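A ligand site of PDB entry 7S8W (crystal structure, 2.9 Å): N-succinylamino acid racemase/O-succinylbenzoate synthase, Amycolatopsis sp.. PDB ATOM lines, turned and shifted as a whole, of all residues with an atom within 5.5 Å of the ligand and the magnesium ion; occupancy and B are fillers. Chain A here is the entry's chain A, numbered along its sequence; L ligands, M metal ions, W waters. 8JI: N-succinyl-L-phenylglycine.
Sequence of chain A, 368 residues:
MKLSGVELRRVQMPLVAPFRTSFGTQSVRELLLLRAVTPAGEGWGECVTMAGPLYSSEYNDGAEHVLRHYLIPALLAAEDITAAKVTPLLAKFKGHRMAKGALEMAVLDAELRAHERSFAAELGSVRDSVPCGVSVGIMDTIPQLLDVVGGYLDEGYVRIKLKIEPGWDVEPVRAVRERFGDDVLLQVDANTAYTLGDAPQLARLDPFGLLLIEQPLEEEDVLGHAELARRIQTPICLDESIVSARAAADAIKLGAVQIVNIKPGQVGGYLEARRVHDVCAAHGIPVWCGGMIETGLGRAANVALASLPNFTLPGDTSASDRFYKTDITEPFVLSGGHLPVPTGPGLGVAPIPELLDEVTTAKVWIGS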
ATOM      1  N   PHE A  19      17.602 -11.491 -14.100  1.00  0.00           N
ATOM      2  CA  PHE A  19      17.606 -12.265 -15.336  1.00  0.00           C
ATOM      3  C   PHE A  19      16.934 -13.597 -15.048  1.00  0.00           C
ATOM      4  O   PHE A  19      17.461 -14.402 -14.282  1.00  0.00           O
ATOM      5  CB  PHE A  19      19.046 -12.442 -15.835  1.00  0.00           C
ATOM      6  CG  PHE A  19      19.159 -13.148 -17.145  1.00  0.00           C
ATOM      7  CD1 PHE A  19      18.582 -12.608 -18.287  1.00  0.00           C
ATOM      8  CD2 PHE A  19      19.860 -14.335 -17.261  1.00  0.00           C
ATOM      9  CE1 PHE A  19      18.673 -13.253 -19.501  1.00  0.00           C
ATOM     10  CE2 PHE A  19      19.962 -14.975 -18.471  1.00  0.00           C
ATOM     11  CZ  PHE A  19      19.370 -14.433 -19.596  1.00  0.00           C
ATOM     12  N   THR A  21      15.289 -17.297 -16.117  1.00  0.00           N
ATOM     13  CA  THR A  21      15.289 -18.407 -17.051  1.00  0.00           C
ATOM     14  C   THR A  21      14.422 -19.516 -16.477  1.00  0.00           C
ATOM     15  O   THR A  21      13.994 -19.457 -15.324  1.00  0.00           O
ATOM     16  CB  THR A  21      16.700 -18.955 -17.292  1.00  0.00           C
ATOM     17  OG1 THR A  21      17.195 -19.511 -16.061  1.00  0.00           O
ATOM     18  CG2 THR A  21      17.642 -17.848 -17.771  1.00  0.00           C
ATOM     19  N   PHE A  23      15.006 -22.067 -15.145  1.00  0.00           N
ATOM     20  CA  PHE A  23      15.510 -22.705 -13.943  1.00  0.00           C
ATOM     21  C   PHE A  23      15.825 -21.716 -12.826  1.00  0.00           C
ATOM     22  O   PHE A  23      16.413 -22.112 -11.819  1.00  0.00           O
ATOM     23  CB  PHE A  23      16.777 -23.527 -14.242  1.00  0.00           C
ATOM     24  CG  PHE A  23      17.953 -22.700 -14.719  1.00  0.00           C
ATOM     25  CD1 PHE A  23      18.758 -22.012 -13.822  1.00  0.00           C
ATOM     26  CD2 PHE A  23      18.235 -22.604 -16.063  1.00  0.00           C
ATOM     27  CE1 PHE A  23      19.817 -21.241 -14.268  1.00  0.00           C
ATOM     28  CE2 PHE A  23      19.303 -21.845 -16.519  1.00  0.00           C
ATOM     29  CZ  PHE A  23      20.093 -21.164 -15.616  1.00  0.00           C
ATOM     30  N   GLN A  26      18.327 -14.904 -11.724  1.00  0.00           N
ATOM     31  CA  GLN A  26      19.632 -14.514 -11.264  1.00  0.00           C
ATOM     32  C   GLN A  26      19.645 -13.031 -11.097  1.00  0.00           C
ATOM     33  O   GLN A  26      19.172 -12.319 -11.954  1.00  0.00           O
ATOM     34  CB  GLN A  26      20.659 -14.888 -12.301  1.00  0.00           C
ATOM     35  CG  GLN A  26      21.307 -16.238 -12.096  1.00  0.00           C
ATOM     36  CD  GLN A  26      22.769 -16.229 -12.449  1.00  0.00           C
ATOM     37  OE1 GLN A  26      23.610 -15.831 -11.652  1.00  0.00           O
ATOM     38  NE2 GLN A  26      23.078 -16.644 -13.662  1.00  0.00           N
ATOM     39  N   MET A  50      27.982 -21.372 -11.825  1.00  0.00           N
ATOM     40  CA  MET A  50      27.177 -20.525 -10.965  1.00  0.00           C
ATOM     41  C   MET A  50      27.277 -21.033  -9.530  1.00  0.00           C
ATOM     42  O   MET A  50      28.020 -21.974  -9.222  1.00  0.00           O
ATOM     43  CB  MET A  50      25.712 -20.482 -11.405  1.00  0.00           C
ATOM     44  CG  MET A  50      25.507 -20.574 -12.888  1.00  0.00           C
ATOM     45  SD  MET A  50      23.970 -19.742 -13.341  1.00  0.00           S
ATOM     46  CE  MET A  50      22.779 -20.736 -12.437  1.00  0.00           C
ATOM     47  N   TYR A  55      22.200 -25.101 -13.550  1.00  0.00           N
ATOM     48  CA  TYR A  55      22.363 -25.126 -14.998  1.00  0.00           C
ATOM     49  C   TYR A  55      23.060 -26.404 -15.463  1.00  0.00           C
ATOM     50  O   TYR A  55      22.696 -26.977 -16.498  1.00  0.00           O
ATOM     51  CB  TYR A  55      23.138 -23.887 -15.446  1.00  0.00           C
ATOM     52  CG  TYR A  55      23.579 -23.904 -16.895  1.00  0.00           C
ATOM     53  CD1 TYR A  55      24.819 -24.426 -17.246  1.00  0.00           C
ATOM     54  CD2 TYR A  55      22.787 -23.371 -17.891  1.00  0.00           C
ATOM     55  CE1 TYR A  55      25.232 -24.455 -18.557  1.00  0.00           C
ATOM     56  CE2 TYR A  55      23.185 -23.392 -19.216  1.00  0.00           C
ATOM     57  CZ  TYR A  55      24.410 -23.936 -19.543  1.00  0.00           C
ATOM     58  OH  TYR A  55      24.820 -23.951 -20.864  1.00  0.00           O
ATOM     59  N   SER A 135      20.169 -11.288 -24.939  1.00  0.00           N
ATOM     60  CA  SER A 135      19.350 -12.350 -24.355  1.00  0.00           C
ATOM     61  C   SER A 135      18.454 -11.724 -23.288  1.00  0.00           C
ATOM     62  O   SER A 135      18.954 -11.174 -22.299  1.00  0.00           O
ATOM     63  CB  SER A 135      20.244 -13.435 -23.769  1.00  0.00           C
ATOM     64  OG  SER A 135      19.486 -14.428 -23.104  1.00  0.00           O
ATOM     65  N   LYS A 161      16.951 -12.500 -28.358  1.00  0.00           N
ATOM     66  CA  LYS A 161      16.783 -13.886 -27.928  1.00  0.00           C
ATOM     67  C   LYS A 161      15.901 -13.872 -26.695  1.00  0.00           C
ATOM     68  O   LYS A 161      16.157 -13.102 -25.761  1.00  0.00           O
ATOM     69  CB  LYS A 161      18.144 -14.531 -27.628  1.00  0.00           C
ATOM     70  CG  LYS A 161      18.136 -15.660 -26.612  1.00  0.00           C
ATOM     71  CD  LYS A 161      19.539 -16.223 -26.447  1.00  0.00           C
ATOM     72  CE  LYS A 161      19.644 -17.171 -25.257  1.00  0.00           C
ATOM     73  NZ  LYS A 161      20.931 -17.933 -25.279  1.00  0.00           N
ATOM     74  N   LYS A 163      14.229 -15.887 -23.545  1.00  0.00           N
ATOM     75  CA  LYS A 163      14.148 -17.086 -22.738  1.00  0.00           C
ATOM     76  C   LYS A 163      12.685 -17.505 -22.608  1.00  0.00           C
ATOM     77  O   LYS A 163      11.816 -16.679 -22.274  1.00  0.00           O
ATOM     78  CB  LYS A 163      14.777 -16.845 -21.373  1.00  0.00           C
ATOM     79  CG  LYS A 163      16.248 -16.570 -21.488  1.00  0.00           C
ATOM     80  CD  LYS A 163      16.999 -17.859 -21.697  1.00  0.00           C
ATOM     81  CE  LYS A 163      18.447 -17.654 -21.429  1.00  0.00           C
ATOM     82  NZ  LYS A 163      19.005 -18.821 -20.721  1.00  0.00           N
ATOM     83  N   ASP A 189      15.104 -19.516 -26.263  1.00  0.00           N
ATOM     84  CA  ASP A 189      15.948 -20.458 -25.526  1.00  0.00           C
ATOM     85  C   ASP A 189      15.136 -20.992 -24.344  1.00  0.00           C
ATOM     86  O   ASP A 189      14.584 -20.205 -23.575  1.00  0.00           O
ATOM     87  CB  ASP A 189      17.231 -19.765 -25.043  1.00  0.00           C
ATOM     88  CG  ASP A 189      18.256 -20.732 -24.455  1.00  0.00           C
ATOM     89  OD1 ASP A 189      17.931 -21.930 -24.256  1.00  0.00           O
ATOM     90  OD2 ASP A 189      19.392 -20.292 -24.164  1.00  0.00           O
ATOM     91  N   ASN A 191      16.257 -23.762 -22.145  1.00  0.00           N
ATOM     92  CA  ASN A 191      17.081 -24.326 -21.059  1.00  0.00           C
ATOM     93  C   ASN A 191      16.530 -25.660 -20.557  1.00  0.00           C
ATOM     94  O   ASN A 191      16.397 -25.890 -19.354  1.00  0.00           O
ATOM     95  CB  ASN A 191      17.221 -23.319 -19.918  1.00  0.00           C
ATOM     96  CG  ASN A 191      18.248 -22.248 -20.219  1.00  0.00           C
ATOM     97  OD1 ASN A 191      17.950 -21.056 -20.172  1.00  0.00           O
ATOM     98  ND2 ASN A 191      19.463 -22.671 -20.544  1.00  0.00           N
ATOM     99  N   GLU A 214      16.539 -22.891 -28.950  1.00  0.00           N
ATOM    100  CA  GLU A 214      17.746 -23.306 -28.256  1.00  0.00           C
ATOM    101  C   GLU A 214      17.419 -24.274 -27.124  1.00  0.00           C
ATOM    102  O   GLU A 214      16.607 -23.964 -26.252  1.00  0.00           O
ATOM    103  CB  GLU A 214      18.462 -22.092 -27.705  1.00  0.00           C
ATOM    104  CG  GLU A 214      19.931 -22.300 -27.443  1.00  0.00           C
ATOM    105  CD  GLU A 214      20.543 -21.065 -26.836  1.00  0.00           C
ATOM    106  OE1 GLU A 214      20.119 -19.956 -27.248  1.00  0.00           O
ATOM    107  OE2 GLU A 214      21.423 -21.204 -25.951  1.00  0.00           O
ATOM    108  N   ASP A 239      22.693 -26.272 -27.006  1.00  0.00           N
ATOM    109  CA  ASP A 239      23.548 -25.504 -26.104  1.00  0.00           C
ATOM    110  C   ASP A 239      24.124 -26.407 -25.020  1.00  0.00           C
ATOM    111  O   ASP A 239      25.296 -26.817 -25.104  1.00  0.00           O
ATOM    112  CB  ASP A 239      22.767 -24.342 -25.479  1.00  0.00           C
ATOM    113  CG  ASP A 239      23.616 -23.444 -24.573  1.00  0.00           C
ATOM    114  OD1 ASP A 239      24.844 -23.668 -24.426  1.00  0.00           O
ATOM    115  OD2 ASP A 239      23.046 -22.488 -24.007  1.00  0.00           O
ATOM    116  N   GLU A 240      23.307 -26.717 -24.011  1.00  0.00           N
ATOM    117  CA  GLU A 240      23.748 -27.543 -22.884  1.00  0.00           C
ATOM    118  C   GLU A 240      24.301 -28.892 -23.359  1.00  0.00           C
ATOM    119  O   GLU A 240      25.147 -29.481 -22.669  1.00  0.00           O
ATOM    120  CB  GLU A 240      22.585 -27.785 -21.926  1.00  0.00           C
ATOM    121  CG  GLU A 240      22.265 -26.703 -20.891  1.00  0.00           C
ATOM    122  CD  GLU A 240      21.318 -25.610 -21.387  1.00  0.00           C
ATOM    123  OE1 GLU A 240      21.191 -25.388 -22.615  1.00  0.00           O
ATOM    124  OE2 GLU A 240      20.627 -25.014 -20.526  1.00  0.00           O
ATOM    125  N   ASN A 261      25.347 -23.522 -30.524  1.00  0.00           N
ATOM    126  CA  ASN A 261      25.794 -22.480 -29.592  1.00  0.00           C
ATOM    127  C   ASN A 261      27.083 -22.966 -28.936  1.00  0.00           C
ATOM    128  O   ASN A 261      27.071 -23.968 -28.198  1.00  0.00           O
ATOM    129  CB  ASN A 261      24.681 -22.226 -28.565  1.00  0.00           C
ATOM    130  CG  ASN A 261      25.077 -21.253 -27.447  1.00  0.00           C
ATOM    131  OD1 ASN A 261      26.233 -20.891 -27.266  1.00  0.00           O
ATOM    132  ND2 ASN A 261      24.075 -20.847 -26.682  1.00  0.00           N
ATOM    133  N   LYS A 263      29.625 -22.424 -26.153  1.00  0.00           N
ATOM    134  CA  LYS A 263      30.021 -21.818 -24.884  1.00  0.00           C
ATOM    135  C   LYS A 263      31.383 -22.335 -24.483  1.00  0.00           C
ATOM    136  O   LYS A 263      31.499 -23.507 -24.076  1.00  0.00           O
ATOM    137  CB  LYS A 263      29.016 -22.093 -23.768  1.00  0.00           C
ATOM    138  CG  LYS A 263      27.786 -21.281 -23.901  1.00  0.00           C
ATOM    139  CD  LYS A 263      26.869 -21.749 -22.815  1.00  0.00           C
ATOM    140  CE  LYS A 263      25.569 -20.985 -22.828  1.00  0.00           C
ATOM    141  NZ  LYS A 263      24.660 -21.512 -21.779  1.00  0.00           N
ATOM    142  N   GLY A 290      28.127 -18.245 -27.165  1.00  0.00           N
ATOM    143  CA  GLY A 290      27.197 -18.208 -26.060  1.00  0.00           C
ATOM    144  C   GLY A 290      27.729 -17.420 -24.883  1.00  0.00           C
ATOM    145  O   GLY A 290      28.941 -17.297 -24.675  1.00  0.00           O
ATOM    146  N   GLY A 291      26.811 -16.872 -24.107  1.00  0.00           N
ATOM    147  CA  GLY A 291      27.203 -16.088 -22.951  1.00  0.00           C
ATOM    148  C   GLY A 291      26.895 -16.770 -21.639  1.00  0.00           C
ATOM    149  O   GLY A 291      26.077 -17.681 -21.581  1.00  0.00           O
ATOM    150  N   MET A 292      27.593 -16.351 -20.588  1.00  0.00           N
ATOM    151  CA  MET A 292      27.311 -16.824 -19.241  1.00  0.00           C
ATOM    152  C   MET A 292      27.363 -15.657 -18.252  1.00  0.00           C
ATOM    153  O   MET A 292      27.724 -15.846 -17.076  1.00  0.00           O
ATOM    154  CB  MET A 292      28.278 -17.939 -18.816  1.00  0.00           C
ATOM    155  CG  MET A 292      28.126 -19.253 -19.580  1.00  0.00           C
ATOM    156  SD  MET A 292      26.550 -20.126 -19.332  1.00  0.00           S
ATOM    157  CE  MET A 292      27.058 -21.414 -18.204  1.00  0.00           C
ATOM    158  N   ILE A 293      26.981 -14.457 -18.692  1.00  0.00           N
ATOM    159  CA  ILE A 293      27.029 -13.248 -17.888  1.00  0.00           C
ATOM    160  C   ILE A 293      28.444 -13.117 -17.335  1.00  0.00           C
ATOM    161  O   ILE A 293      28.638 -13.025 -16.119  1.00  0.00           O
ATOM    162  CB  ILE A 293      25.980 -13.252 -16.760  1.00  0.00           C
ATOM    163  CG1 ILE A 293      24.658 -13.871 -17.235  1.00  0.00           C
ATOM    164  CG2 ILE A 293      25.691 -11.839 -16.282  1.00  0.00           C
ATOM    165  CD1 ILE A 293      23.630 -13.983 -16.136  1.00  0.00           C
ATOM    166  N   GLU A 294      29.432 -13.147 -18.222  1.00  0.00           N
ATOM    167  CA  GLU A 294      30.809 -13.107 -17.787  1.00  0.00           C
ATOM    168  C   GLU A 294      31.255 -11.665 -17.528  1.00  0.00           C
ATOM    169  O   GLU A 294      30.601 -10.698 -17.932  1.00  0.00           O
ATOM    170  CB  GLU A 294      31.744 -13.729 -18.831  1.00  0.00           C
ATOM    171  CG  GLU A 294      31.576 -15.225 -19.056  1.00  0.00           C
ATOM    172  CD  GLU A 294      31.028 -15.513 -20.424  1.00  0.00           C
ATOM    173  OE1 GLU A 294      30.127 -14.751 -20.855  1.00  0.00           O
ATOM    174  OE2 GLU A 294      31.475 -16.475 -21.079  1.00  0.00           O
ATOM    175  N   ARG A 299      34.269 -11.949 -21.443  1.00  0.00           N
ATOM    176  CA  ARG A 299      33.640 -11.237 -22.556  1.00  0.00           C
ATOM    177  C   ARG A 299      34.648 -10.946 -23.659  1.00  0.00           C
ATOM    178  O   ARG A 299      34.319 -11.032 -24.851  1.00  0.00           O
ATOM    179  CB  ARG A 299      32.985  -9.946 -22.066  1.00  0.00           C
ATOM    180  CG  ARG A 299      32.131  -9.255 -23.103  1.00  0.00           C
ATOM    181  CD  ARG A 299      31.134  -8.283 -22.472  1.00  0.00           C
ATOM    182  NE  ARG A 299      30.399  -8.898 -21.373  1.00  0.00           N
ATOM    183  CZ  ARG A 299      29.304  -9.630 -21.521  1.00  0.00           C
ATOM    184  NH1 ARG A 299      28.810  -9.851 -22.738  1.00  0.00           N
ATOM    185  NH2 ARG A 299      28.716 -10.144 -20.460  1.00  0.00           N
ATOM    186  N   ASP A 316      25.643 -14.061 -28.176  1.00  0.00           N
ATOM    187  CA  ASP A 316      25.285 -13.464 -26.889  1.00  0.00           C
ATOM    188  C   ASP A 316      26.481 -12.702 -26.350  1.00  0.00           C
ATOM    189  O   ASP A 316      26.878 -12.866 -25.191  1.00  0.00           O
ATOM    190  CB  ASP A 316      24.860 -14.543 -25.885  1.00  0.00           C
ATOM    191  CG  ASP A 316      23.460 -15.079 -26.140  1.00  0.00           C
ATOM    192  OD1 ASP A 316      22.672 -14.415 -26.866  1.00  0.00           O
ATOM    193  OD2 ASP A 316      23.146 -16.181 -25.621  1.00  0.00           O
ATOM    194  N   THR A 317      27.089 -11.886 -27.208  1.00  0.00           N
ATOM    195  CA  THR A 317      28.232 -11.057 -26.843  1.00  0.00           C
ATOM    196  C   THR A 317      27.766  -9.607 -26.655  1.00  0.00           C
ATOM    197  O   THR A 317      28.165  -8.702 -27.374  1.00  0.00           O
ATOM    198  CB  THR A 317      29.326 -11.179 -27.901  1.00  0.00           C
ATOM    199  OG1 THR A 317      28.746 -11.058 -29.225  1.00  0.00           O
ATOM    200  CG2 THR A 317      30.020 -12.531 -27.798  1.00  0.00           C
ATOM    201  N   SER A 318      26.928  -9.418 -25.639  1.00  0.00           N
ATOM    202  CA  SER A 318      26.359  -8.103 -25.373  1.00  0.00           C
ATOM    203  C   SER A 318      27.406  -7.168 -24.770  1.00  0.00           C
ATOM    204  O   SER A 318      28.526  -7.567 -24.405  1.00  0.00           O
ATOM    205  CB  SER A 318      25.159  -8.214 -24.419  1.00  0.00           C
ATOM    206  OG  SER A 318      24.070  -8.902 -25.012  1.00  0.00           O
ATOM    207  N   PHE A 323      24.517  -5.829 -18.293  1.00  0.00           N
ATOM    208  CA  PHE A 323      24.599  -6.662 -17.105  1.00  0.00           C
ATOM    209  C   PHE A 323      25.213  -5.898 -15.940  1.00  0.00           C
ATOM    210  O   PHE A 323      24.716  -6.014 -14.820  1.00  0.00           O
ATOM    211  CB  PHE A 323      25.337  -8.004 -17.252  1.00  0.00           C
ATOM    212  CG  PHE A 323      24.544  -9.045 -17.981  1.00  0.00           C
ATOM    213  CD1 PHE A 323      23.323  -9.462 -17.495  1.00  0.00           C
ATOM    214  CD2 PHE A 323      25.036  -9.615 -19.151  1.00  0.00           C
ATOM    215  CE1 PHE A 323      22.585 -10.437 -18.168  1.00  0.00           C
ATOM    216  CE2 PHE A 323      24.316 -10.574 -19.827  1.00  0.00           C
ATOM    217  CZ  PHE A 323      23.092 -10.992 -19.331  1.00  0.00           C
HETATM  218  C15 8JI L   1      23.510 -14.363 -21.405  1.00  0.00           C
HETATM  219  C01 8JI L   1      22.399 -18.594 -16.854  1.00  0.00           C
HETATM  220  C02 8JI L   1      22.192 -17.495 -17.665  1.00  0.00           C
HETATM  221  C03 8JI L   1      22.406 -17.588 -19.023  1.00  0.00           C
HETATM  222  C04 8JI L   1      22.833 -18.786 -19.558  1.00  0.00           C
HETATM  223  C05 8JI L   1      23.052 -19.879 -18.742  1.00  0.00           C
HETATM  224  C06 8JI L   1      22.839 -19.785 -17.384  1.00  0.00           C
HETATM  225  C07 8JI L   1      23.098 -18.873 -21.067  1.00  0.00           C
HETATM  226  C08 8JI L   1      22.080 -19.748 -21.832  1.00  0.00           C
HETATM  227  C12 8JI L   1      22.435 -16.528 -22.040  1.00  0.00           C
HETATM  228  C14 8JI L   1      23.012 -15.220 -22.559  1.00  0.00           C
HETATM  229  C16 8JI L   1      24.678 -13.468 -21.792  1.00  0.00           C
HETATM  230  N11 8JI L   1      23.373 -17.538 -21.610  1.00  0.00           N
HETATM  231  O09 8JI L   1      21.314 -20.493 -21.159  1.00  0.00           O
HETATM  232  O10 8JI L   1      22.029 -19.780 -23.092  1.00  0.00           O
HETATM  233  O13 8JI L   1      21.260 -16.707 -22.003  1.00  0.00           O
HETATM  234  O17 8JI L   1      25.773 -13.601 -21.189  1.00  0.00           O
HETATM  235  O18 8JI L   1      24.546 -12.608 -22.696  1.00  0.00           O
HETATM  236 MG    MG M   1      21.382 -21.230 -23.790  1.00  0.00          MG
HETATM  237  O   HOH W   1      23.843 -18.650 -24.528  1.00  0.00           O
HETATM  238  O   HOH W   2      20.222 -23.107 -23.866  1.00  0.00           O
HETATM  239  O   HOH W   3      24.984 -18.362 -15.466  1.00  0.00           O
HETATM  240  O   HOH W   4      28.364 -12.783 -21.636  1.00  0.00           O
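The side-chain hydroxyl (OG) of Ser 135 lies within hydrogen-bond range of an oxygen (O13) of the ligand, 3.1 Å away.
O09 of the ligand is in hydrogen-bond range of ND2 of Asn 191 (2.9 Å).
The backbone NH (N) of Met 292 lies within hydrogen-bond range of an oxygen (O17) of the ligand (3.4 Å).
An oxygen (O09) of the ligand is in salt-bridge range of the side-chain amino group (NZ) of Lys 163 (2.9 Å).
N of Ile 293 lies within hydrogen-bond range of O17 of the ligand, 2.9 Å away.
The side-chain amino group (NZ) of Lys 161 sits close to an oxygen (O10) of the ligand (3.1 Å).
The backbone carbonyl oxygen (O) of Gly 291 is in hydrogen-bond range of a nitrogen (N11) of the ligand (2.7 Å).
An oxygen (O09) of the ligand lies within salt-bridge range of the side-chain amino group (NZ) of Lys 263, 3.6 Å away.
The side-chain carboxylate of Asp 189 is in hydrogen-bond range of the backbone NH of Asn 191 (3.3 Å).
NZ of Lys 263 lies within hydrogen-bond range of SD of Met 292.
The backbone NH of Phe 23 lies close to the side-chain hydroxyl of Thr 21, at 3.5 Å.
The side-chain amide oxygen (OD1) of Asn 261 sits close to the backbone NH (N) of Gly 290, at 3.3 Å.
The backbone NH (N) of Met 292 sits at hydrogen-bond distance from the side-chain carboxylate (OE1) of Glu 294 (3.0 Å).
OE1 of Glu 214 lies within salt-bridge range of NZ of Lys 161 (2.9 Å).
The side-chain amide nitrogen of Asn 191 is in hydrogen-bond range of the side-chain carboxylate of Glu 240 (2.6 Å).
The side-chain amide oxygen (OD1) of Asn 191 lies within hydrogen-bond range of the side-chain amino group (NZ) of Lys 163 (2.5 Å).
An oxygen (O18) of the ligand lies close to the backbone carbonyl oxygen of Asp 316, at 3.4 Å.
Phe 19 touches the ligand (CE2 to C02, 3.5 Å).
Phe 23 touches the ligand.
NE2 of Gln 26 touches C01 of the ligand, at 3.8 Å.
Tyr 55 touches the ligand.
CE2 of Phe 323 touches C16 of the ligand, at 3.5 Å.
Hydrophobic or aromatic side chains within 4 Å of the ligand: Phe 19, Phe 23, Tyr 55, Met 292 and Phe 323.
The nearest printed residue that does not touch the ligand is Met 50 (4.02 Å).
Merely in contact with the magnesium ion: Lys 161 (3.6 Å), Lys 263 (3.9 Å) and Asn 261 (3.97 Å).
Six residues have an atom within 4 Å of the magnesium ion: Lys 161, Asp 189, Glu 214, Asp 239, Asn 261 and Lys 263.
The nearest printed residue that does not touch the magnesium ion is Asn 191 (4.04 Å).
The magnesium ion is bound by O10 of the ligand (1.7 Å), OD2 of Asp 239 (2.1 Å), OE2 of Glu 214 (2.2 Å), water W2 (2.2 Å) and OD2 of Asp 189 (2.2 Å).
Slightly farther from the magnesium ion lies O09 of the ligand (2.7 Å).
Water W2 lies within hydrogen-bond range of the side-chain carboxylate (OD1) of Asp 189 (2.6 Å), the side-chain carboxylate (OE1) of Glu 240 (2.8 Å) and the side-chain amide nitrogen (ND2) of Asn 191 (3.4 Å).
Water W4 lies within hydrogen-bond range of an oxygen (O17) of the ligand (2.8 Å), the side-chain carboxylate (OE1) of Glu 294 (2.8 Å) and the guanidinium group (NH2) of Arg 299 (2.9 Å).
Water W3 bridges the side-chain sulfur of Met 50 (2.7 Å) and the side-chain amide nitrogen of Gln 26 (3.1 Å).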
